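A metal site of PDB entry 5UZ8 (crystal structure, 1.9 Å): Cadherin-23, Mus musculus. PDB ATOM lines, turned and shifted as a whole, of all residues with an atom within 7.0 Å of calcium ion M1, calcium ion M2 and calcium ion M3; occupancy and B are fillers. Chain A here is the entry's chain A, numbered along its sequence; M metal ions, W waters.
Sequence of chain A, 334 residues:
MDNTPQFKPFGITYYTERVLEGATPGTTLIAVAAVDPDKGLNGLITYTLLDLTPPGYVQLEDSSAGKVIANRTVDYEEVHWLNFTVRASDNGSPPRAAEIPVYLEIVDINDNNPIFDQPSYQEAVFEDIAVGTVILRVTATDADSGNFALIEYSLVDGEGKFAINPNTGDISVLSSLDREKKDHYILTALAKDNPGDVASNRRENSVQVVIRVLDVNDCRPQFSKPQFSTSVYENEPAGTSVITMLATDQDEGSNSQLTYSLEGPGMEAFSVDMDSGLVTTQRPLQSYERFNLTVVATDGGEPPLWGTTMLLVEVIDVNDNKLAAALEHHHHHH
Six residues have an atom within 4 Å of calcium ion M2: Asn 110, Asn 112, Asp 142, Asp 144, Phe 148 and Asp 193.
Within 4 Å of calcium ion M3: Glu 21, Asp 75, Glu 77 and Asp 111. The nearest printed residue that does not touch calcium ion M3 is Asn 112 (4.1 Å).
O of Asn 110 is in hydrogen-bond range of NE of Arg 203 (2.8 Å). The backbone carbonyl oxygen (O) of Asn 201 is in hydrogen-bond range of the side-chain amide nitrogen (ND2) of Asn 110. The side-chain carboxylate (OD1) of Asp 111 lies close to the side-chain amide nitrogen (ND2) of Asn 112, 3.2 Å away. The backbone NH of Arg 203 sits at hydrogen-bond distance from the side-chain carboxylate of Asp 193 (2.8 Å). The side-chain carboxylate (OD2) of Asp 108 is in hydrogen-bond range of the backbone NH (N) of Ser 145 (3.0 Å). The side-chain amide nitrogen (ND2) of Asn 112 lies close to the side-chain carboxylate (OE2) of Glu 77, 3.2 Å away. The backbone NH (N) of Glu 21 is in hydrogen-bond range of the backbone carbonyl oxygen (O) of Val 107. The side-chain carboxylate (OE2) of Glu 21 lies close to the backbone NH (N) of Tyr 76.
Of the 27 residues printed, 7 come within 4 Å of calcium ion M1. Along chain A the residues within 4 Å of calcium ion M1 span positions 21 to 144.
Calcium ion M1 is bound by OD1 of Asp 108 (2.2 Å), OD1 of Asp 144 (2.3 Å), OE1 of Glu 21 (2.3 Å), OD1 of Asp 111 (2.4 Å), O of Ile 109 (2.5 Å), OE1 of Glu 77 (2.5 Å) and OE2 of Glu 77 (2.6 Å). Calcium ion M1 has seven donor atoms within binding distance.
Calcium ion M3 is bound by OE2 of Glu 77 (2.3 Å), OD2 of Asp 111 (2.3 Å), OD1 of Asp 75 (2.4 Å), water W1 (2.4 Å), OE2 of Glu 21 (2.4 Å) and water W2 (2.4 Å). Calcium ion M3 has six donor atoms within binding distance. Slightly farther from calcium ion M3 lies the side-chain carboxylate (OD1) of Asp 111 (3.1 Å).
Calcium ion M2 is bound by O of Asn 112, OD2 of Asp 193, OD1 of Asn 110, OD2 of Asp 144, O of Phe 148, OD2 of Asp 142 and OD1 of Asp 142. Calcium ion M2 has seven donor atoms within binding distance.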
ATOM      1  N   GLU A  21       2.705  19.429 -30.232  1.00  0.00           N
ATOM      2  CA  GLU A  21       3.926  19.711 -30.993  1.00  0.00           C
ATOM      3  C   GLU A  21       4.965  18.621 -30.749  1.00  0.00           C
ATOM      4  O   GLU A  21       5.004  18.010 -29.675  1.00  0.00           O
ATOM      5  CB  GLU A  21       4.487  21.094 -30.678  1.00  0.00           C
ATOM      6  CG  GLU A  21       5.035  21.234 -29.273  1.00  0.00           C
ATOM      7  CD  GLU A  21       5.862  22.486 -29.087  1.00  0.00           C
ATOM      8  OE1 GLU A  21       5.813  23.069 -27.968  1.00  0.00           O
ATOM      9  OE2 GLU A  21       6.579  22.855 -30.034  1.00  0.00           O
ATOM     10  N   GLY A  22       5.750  18.314 -31.769  1.00  0.00           N
ATOM     11  CA  GLY A  22       6.762  17.287 -31.692  1.00  0.00           C
ATOM     12  C   GLY A  22       6.307  15.879 -31.992  1.00  0.00           C
ATOM     13  O   GLY A  22       7.131  14.959 -31.952  1.00  0.00           O
ATOM     14  N   VAL A  74       5.875  19.137 -36.265  1.00  0.00           N
ATOM     15  CA  VAL A  74       5.429  20.526 -36.107  1.00  0.00           C
ATOM     16  C   VAL A  74       5.981  21.105 -34.805  1.00  0.00           C
ATOM     17  O   VAL A  74       6.146  20.379 -33.803  1.00  0.00           O
ATOM     18  CB  VAL A  74       3.892  20.614 -36.166  1.00  0.00           C
ATOM     19  CG1 VAL A  74       3.235  20.074 -34.909  1.00  0.00           C
ATOM     20  CG2 VAL A  74       3.434  22.029 -36.465  1.00  0.00           C
ATOM     21  N   ASP A  75       6.263  22.388 -34.850  1.00  0.00           N
ATOM     22  CA  ASP A  75       6.812  23.163 -33.754  1.00  0.00           C
ATOM     23  C   ASP A  75       5.792  24.259 -33.375  1.00  0.00           C
ATOM     24  O   ASP A  75       5.514  25.145 -34.177  1.00  0.00           O
ATOM     25  CB  ASP A  75       8.117  23.802 -34.226  1.00  0.00           C
ATOM     26  CG  ASP A  75       8.825  24.622 -33.136  1.00  0.00           C
ATOM     27  OD1 ASP A  75       8.368  24.677 -31.976  1.00  0.00           O
ATOM     28  OD2 ASP A  75       9.854  25.223 -33.461  1.00  0.00           O
ATOM     29  N   TYR A  76       5.261  24.216 -32.158  1.00  0.00           N
ATOM     30  CA  TYR A  76       4.307  25.208 -31.687  1.00  0.00           C
ATOM     31  C   TYR A  76       4.916  26.595 -31.763  1.00  0.00           C
ATOM     32  O   TYR A  76       4.212  27.552 -32.012  1.00  0.00           O
ATOM     33  CB  TYR A  76       3.853  24.918 -30.243  1.00  0.00           C
ATOM     34  CG  TYR A  76       2.808  25.885 -29.762  1.00  0.00           C
ATOM     35  CD1 TYR A  76       1.435  25.696 -30.087  1.00  0.00           C
ATOM     36  CD2 TYR A  76       3.150  27.017 -29.023  1.00  0.00           C
ATOM     37  CE1 TYR A  76       0.483  26.595 -29.653  1.00  0.00           C
ATOM     38  CE2 TYR A  76       2.189  27.886 -28.589  1.00  0.00           C
ATOM     39  CZ  TYR A  76       0.881  27.681 -28.916  1.00  0.00           C
ATOM     40  OH  TYR A  76      -0.054  28.582 -28.482  1.00  0.00           O
ATOM     41  N   GLU A  77       6.221  26.707 -31.546  1.00  0.00           N
ATOM     42  CA  GLU A  77       6.867  28.000 -31.621  1.00  0.00           C
ATOM     43  C   GLU A  77       6.889  28.590 -33.052  1.00  0.00           C
ATOM     44  O   GLU A  77       7.181  29.763 -33.195  1.00  0.00           O
ATOM     45  CB  GLU A  77       8.250  27.967 -30.976  1.00  0.00           C
ATOM     46  CG  GLU A  77       8.229  27.979 -29.454  1.00  0.00           C
ATOM     47  CD  GLU A  77       7.585  26.753 -28.791  1.00  0.00           C
ATOM     48  OE1 GLU A  77       6.623  26.984 -28.063  1.00  0.00           O
ATOM     49  OE2 GLU A  77       8.037  25.587 -28.950  1.00  0.00           O
ATOM     50  N   GLU A  78       6.535  27.773 -34.075  1.00  0.00           N
ATOM     51  CA  GLU A  78       6.429  28.233 -35.478  1.00  0.00           C
ATOM     52  C   GLU A  78       4.993  28.195 -36.000  1.00  0.00           C
ATOM     53  O   GLU A  78       4.620  29.044 -36.803  1.00  0.00           O
ATOM     54  CB  GLU A  78       7.291  27.344 -36.389  1.00  0.00           C
ATOM     55  CG  GLU A  78       8.775  27.444 -36.106  1.00  0.00           C
ATOM     56  CD  GLU A  78       9.308  28.855 -36.285  1.00  0.00           C
ATOM     57  OE1 GLU A  78       8.678  29.648 -37.023  1.00  0.00           O
ATOM     58  OE2 GLU A  78      10.342  29.191 -35.683  1.00  0.00           O
ATOM     59  N   VAL A 107      -0.669  22.004 -29.793  1.00  0.00           N
ATOM     60  CA  VAL A 107      -0.606  22.186 -28.345  1.00  0.00           C
ATOM     61  C   VAL A 107       0.848  22.376 -27.953  1.00  0.00           C
ATOM     62  O   VAL A 107       1.710  21.579 -28.333  1.00  0.00           O
ATOM     63  CB  VAL A 107      -1.157  20.961 -27.637  1.00  0.00           C
ATOM     64  CG1 VAL A 107      -1.037  21.090 -26.116  1.00  0.00           C
ATOM     65  CG2 VAL A 107      -2.608  20.744 -28.037  1.00  0.00           C
ATOM     66  N   ASP A 108       1.107  23.451 -27.217  1.00  0.00           N
ATOM     67  CA  ASP A 108       2.451  23.765 -26.726  1.00  0.00           C
ATOM     68  C   ASP A 108       2.880  22.714 -25.707  1.00  0.00           C
ATOM     69  O   ASP A 108       2.112  22.344 -24.797  1.00  0.00           O
ATOM     70  CB  ASP A 108       2.385  25.142 -26.054  1.00  0.00           C
ATOM     71  CG  ASP A 108       3.719  25.650 -25.522  1.00  0.00           C
ATOM     72  OD1 ASP A 108       4.790  25.421 -26.153  1.00  0.00           O
ATOM     73  OD2 ASP A 108       3.669  26.380 -24.495  1.00  0.00           O
ATOM     74  N   ILE A 109       4.123  22.268 -25.818  1.00  0.00           N
ATOM     75  CA  ILE A 109       4.794  21.511 -24.746  1.00  0.00           C
ATOM     76  C   ILE A 109       5.969  22.328 -24.224  1.00  0.00           C
ATOM     77  O   ILE A 109       6.439  23.269 -24.875  1.00  0.00           O
ATOM     78  CB  ILE A 109       5.262  20.093 -25.194  1.00  0.00           C
ATOM     79  CG1 ILE A 109       6.513  20.167 -26.066  1.00  0.00           C
ATOM     80  CG2 ILE A 109       4.130  19.332 -25.888  1.00  0.00           C
ATOM     81  CD1 ILE A 109       7.015  18.829 -26.598  1.00  0.00           C
ATOM     82  N   ASN A 110       6.448  21.987 -23.036  1.00  0.00           N
ATOM     83  CA  ASN A 110       7.500  22.733 -22.413  1.00  0.00           C
ATOM     84  C   ASN A 110       8.858  22.254 -22.899  1.00  0.00           C
ATOM     85  O   ASN A 110       9.611  21.587 -22.172  1.00  0.00           O
ATOM     86  CB  ASN A 110       7.405  22.661 -20.881  1.00  0.00           C
ATOM     87  CG  ASN A 110       8.346  23.632 -20.198  1.00  0.00           C
ATOM     88  OD1 ASN A 110       8.724  24.629 -20.792  1.00  0.00           O
ATOM     89  ND2 ASN A 110       8.715  23.356 -18.962  1.00  0.00           N
ATOM     90  N   ASP A 111       9.176  22.635 -24.142  1.00  0.00           N
ATOM     91  CA  ASP A 111      10.415  22.201 -24.809  1.00  0.00           C
ATOM     92  C   ASP A 111      11.489  23.294 -24.935  1.00  0.00           C
ATOM     93  O   ASP A 111      12.521  23.050 -25.578  1.00  0.00           O
ATOM     94  CB  ASP A 111      10.115  21.506 -26.150  1.00  0.00           C
ATOM     95  CG  ASP A 111       9.382  22.383 -27.173  1.00  0.00           C
ATOM     96  OD1 ASP A 111       8.761  23.420 -26.828  1.00  0.00           O
ATOM     97  OD2 ASP A 111       9.336  21.974 -28.357  1.00  0.00           O
ATOM     98  N   ASN A 112      11.280  24.447 -24.324  1.00  0.00           N
ATOM     99  CA  ASN A 112      12.306  25.484 -24.300  1.00  0.00           C
ATOM    100  C   ASN A 112      12.679  25.834 -22.855  1.00  0.00           C
ATOM    101  O   ASN A 112      11.801  26.029 -22.007  1.00  0.00           O
ATOM    102  CB  ASN A 112      11.852  26.742 -25.034  1.00  0.00           C
ATOM    103  CG  ASN A 112      11.770  26.510 -26.544  1.00  0.00           C
ATOM    104  OD1 ASN A 112      12.769  26.666 -27.245  1.00  0.00           O
ATOM    105  ND2 ASN A 112      10.606  26.042 -27.016  1.00  0.00           N
ATOM    106  N   ASN A 113      13.972  25.949 -22.602  1.00  0.00           N
ATOM    107  CA  ASN A 113      14.474  26.368 -21.300  1.00  0.00           C
ATOM    108  C   ASN A 113      14.458  27.881 -21.232  1.00  0.00           C
ATOM    109  O   ASN A 113      14.694  28.524 -22.263  1.00  0.00           O
ATOM    110  CB  ASN A 113      15.928  25.944 -21.106  1.00  0.00           C
ATOM    111  CG  ASN A 113      16.086  24.442 -20.947  1.00  0.00           C
ATOM    112  OD1 ASN A 113      15.591  23.700 -21.745  1.00  0.00           O
ATOM    113  ND2 ASN A 113      16.777  24.013 -19.900  1.00  0.00           N
ATOM    114  N   PRO A 114      14.346  28.442 -20.008  1.00  0.00           N
ATOM    115  CA  PRO A 114      14.696  29.864 -19.881  1.00  0.00           C
ATOM    116  C   PRO A 114      16.165  30.052 -20.164  1.00  0.00           C
ATOM    117  O   PRO A 114      16.992  29.209 -19.764  1.00  0.00           O
ATOM    118  CB  PRO A 114      14.370  30.203 -18.421  1.00  0.00           C
ATOM    119  CG  PRO A 114      13.622  29.062 -17.876  1.00  0.00           C
ATOM    120  CD  PRO A 114      13.978  27.838 -18.729  1.00  0.00           C
ATOM    121  N   ASP A 142      11.937  32.907 -22.238  1.00  0.00           N
ATOM    122  CA  ASP A 142      11.479  31.536 -22.489  1.00  0.00           C
ATOM    123  C   ASP A 142      10.522  31.555 -23.701  1.00  0.00           C
ATOM    124  O   ASP A 142       9.503  32.246 -23.700  1.00  0.00           O
ATOM    125  CB  ASP A 142      10.804  30.988 -21.259  1.00  0.00           C
ATOM    126  CG  ASP A 142      10.543  29.476 -21.334  1.00  0.00           C
ATOM    127  OD1 ASP A 142       9.808  29.032 -22.251  1.00  0.00           O
ATOM    128  OD2 ASP A 142      10.958  28.732 -20.423  1.00  0.00           O
ATOM    129  N   ALA A 143      10.861  30.761 -24.706  1.00  0.00           N
ATOM    130  CA  ALA A 143      10.129  30.726 -25.973  1.00  0.00           C
ATOM    131  C   ALA A 143       8.796  29.970 -26.004  1.00  0.00           C
ATOM    132  O   ALA A 143       8.082  30.059 -26.987  1.00  0.00           O
ATOM    133  CB  ALA A 143      11.068  30.180 -27.063  1.00  0.00           C
ATOM    134  N   ASP A 144       8.425  29.278 -24.922  1.00  0.00           N
ATOM    135  CA  ASP A 144       7.129  28.618 -24.844  1.00  0.00           C
ATOM    136  C   ASP A 144       6.006  29.633 -24.572  1.00  0.00           C
ATOM    137  O   ASP A 144       6.218  30.856 -24.707  1.00  0.00           O
ATOM    138  CB  ASP A 144       7.176  27.500 -23.782  1.00  0.00           C
ATOM    139  CG  ASP A 144       8.193  26.438 -24.126  1.00  0.00           C
ATOM    140  OD1 ASP A 144       8.183  25.945 -25.268  1.00  0.00           O
ATOM    141  OD2 ASP A 144       9.048  26.131 -23.263  1.00  0.00           O
ATOM    142  N   SER A 145       4.841  29.132 -24.223  1.00  0.00           N
ATOM    143  CA  SER A 145       3.667  29.926 -23.966  1.00  0.00           C
ATOM    144  C   SER A 145       3.045  29.578 -22.600  1.00  0.00           C
ATOM    145  O   SER A 145       3.286  28.521 -22.027  1.00  0.00           O
ATOM    146  CB  SER A 145       2.663  29.743 -25.089  1.00  0.00           C
ATOM    147  OG  SER A 145       3.241  30.267 -26.315  1.00  0.00           O
ATOM    148  N   ASN A 147       2.063  28.999 -18.879  1.00  0.00           N
ATOM    149  CA  ASN A 147       2.857  28.636 -17.678  1.00  0.00           C
ATOM    150  C   ASN A 147       4.252  28.118 -18.023  1.00  0.00           C
ATOM    151  O   ASN A 147       5.189  28.355 -17.270  1.00  0.00           O
ATOM    152  CB  ASN A 147       2.156  27.599 -16.799  1.00  0.00           C
ATOM    153  CG  ASN A 147       2.448  27.812 -15.338  1.00  0.00           C
ATOM    154  OD1 ASN A 147       2.018  28.835 -14.796  1.00  0.00           O
ATOM    155  ND2 ASN A 147       3.181  26.901 -14.693  1.00  0.00           N
ATOM    156  N   PHE A 148       4.377  27.459 -19.166  1.00  0.00           N
ATOM    157  CA  PHE A 148       5.644  26.957 -19.627  1.00  0.00           C
ATOM    158  C   PHE A 148       6.681  28.021 -19.936  1.00  0.00           C
ATOM    159  O   PHE A 148       7.873  27.703 -20.093  1.00  0.00           O
ATOM    160  CB  PHE A 148       5.405  26.082 -20.866  1.00  0.00           C
ATOM    161  CG  PHE A 148       4.597  24.852 -20.628  1.00  0.00           C
ATOM    162  CD1 PHE A 148       4.501  24.246 -19.363  1.00  0.00           C
ATOM    163  CD2 PHE A 148       4.007  24.214 -21.700  1.00  0.00           C
ATOM    164  CE1 PHE A 148       3.792  23.072 -19.187  1.00  0.00           C
ATOM    165  CE2 PHE A 148       3.311  23.030 -21.535  1.00  0.00           C
ATOM    166  CZ  PHE A 148       3.189  22.452 -20.270  1.00  0.00           C
ATOM    167  N   ALA A 149       6.252  29.283 -20.039  1.00  0.00           N
ATOM    168  CA  ALA A 149       7.185  30.411 -20.293  1.00  0.00           C
ATOM    169  C   ALA A 149       7.257  31.420 -19.125  1.00  0.00           C
ATOM    170  O   ALA A 149       7.918  32.465 -19.258  1.00  0.00           O
ATOM    171  CB  ALA A 149       6.774  31.129 -21.583  1.00  0.00           C
ATOM    172  N   LEU A 150       6.587  31.106 -18.008  1.00  0.00           N
ATOM    173  CA  LEU A 150       6.705  31.903 -16.811  1.00  0.00           C
ATOM    174  C   LEU A 150       7.965  31.473 -16.091  1.00  0.00           C
ATOM    175  O   LEU A 150       8.226  30.278 -15.986  1.00  0.00           O
ATOM    176  CB  LEU A 150       5.514  31.745 -15.889  1.00  0.00           C
ATOM    177  CG  LEU A 150       4.190  32.235 -16.458  1.00  0.00           C
ATOM    178  CD1 LEU A 150       3.093  32.120 -15.406  1.00  0.00           C
ATOM    179  CD2 LEU A 150       4.343  33.700 -16.899  1.00  0.00           C
ATOM    180  N   ASP A 193      11.396  27.573 -15.245  1.00  0.00           N
ATOM    181  CA  ASP A 193      10.096  27.841 -15.835  1.00  0.00           C
ATOM    182  C   ASP A 193       9.002  27.021 -15.169  1.00  0.00           C
ATOM    183  O   ASP A 193       9.267  26.282 -14.220  1.00  0.00           O
ATOM    184  CB  ASP A 193      10.159  27.682 -17.372  1.00  0.00           C
ATOM    185  CG  ASP A 193      10.282  26.238 -17.809  1.00  0.00           C
ATOM    186  OD1 ASP A 193      10.047  25.307 -17.002  1.00  0.00           O
ATOM    187  OD2 ASP A 193      10.582  26.056 -19.008  1.00  0.00           O
ATOM    188  N   ASN A 194       7.772  27.148 -15.666  1.00  0.00           N
ATOM    189  CA  ASN A 194       6.649  26.281 -15.347  1.00  0.00           C
ATOM    190  C   ASN A 194       6.354  26.171 -13.839  1.00  0.00           C
ATOM    191  O   ASN A 194       6.343  25.077 -13.264  1.00  0.00           O
ATOM    192  CB  ASN A 194       6.845  24.875 -16.008  1.00  0.00           C
ATOM    193  CG  ASN A 194       5.583  24.024 -16.001  1.00  0.00           C
ATOM    194  OD1 ASN A 194       4.459  24.501 -15.857  1.00  0.00           O
ATOM    195  ND2 ASN A 194       5.787  22.695 -16.179  1.00  0.00           N
ATOM    196  N   ASN A 201       8.840  18.438 -15.020  1.00  0.00           N
ATOM    197  CA  ASN A 201       8.332  19.194 -16.190  1.00  0.00           C
ATOM    198  C   ASN A 201       8.760  20.659 -16.086  1.00  0.00           C
ATOM    199  O   ASN A 201       8.250  21.478 -16.806  1.00  0.00           O
ATOM    200  CB  ASN A 201       6.765  19.031 -16.388  1.00  0.00           C
ATOM    201  CG  ASN A 201       6.240  19.390 -17.843  1.00  0.00           C
ATOM    202  OD1 ASN A 201       6.922  19.276 -18.867  1.00  0.00           O
ATOM    203  ND2 ASN A 201       4.984  19.796 -17.897  1.00  0.00           N
ATOM    204  N   ARG A 203      12.007  23.305 -16.571  1.00  0.00           N
ATOM    205  CA  ARG A 203      13.305  23.490 -17.185  1.00  0.00           C
ATOM    206  C   ARG A 203      13.976  24.713 -16.582  1.00  0.00           C
ATOM    207  O   ARG A 203      13.328  25.640 -16.103  1.00  0.00           O
ATOM    208  CB  ARG A 203      13.152  23.691 -18.703  1.00  0.00           C
ATOM    209  CG  ARG A 203      12.772  22.459 -19.463  1.00  0.00           C
ATOM    210  CD  ARG A 203      12.496  22.746 -20.932  1.00  0.00           C
ATOM    211  NE  ARG A 203      12.325  21.514 -21.709  1.00  0.00           N
ATOM    212  CZ  ARG A 203      13.300  20.764 -22.214  1.00  0.00           C
ATOM    213  NH1 ARG A 203      12.994  19.690 -22.915  1.00  0.00           N
ATOM    214  NH2 ARG A 203      14.576  21.090 -22.076  1.00  0.00           N
HETATM  215 CA    CA M   1       6.849  24.806 -26.779  1.00  0.00          CA
HETATM  216 CA    CA M   2       9.814  26.723 -21.086  1.00  0.00          CA
HETATM  217 CA    CA M   3       8.844  23.674 -29.899  1.00  0.00          CA
HETATM  218  O   HOH W   1      10.973  24.675 -29.644  1.00  0.00           O
HETATM  219  O   HOH W   2       9.974  22.189 -31.485  1.00  0.00           O
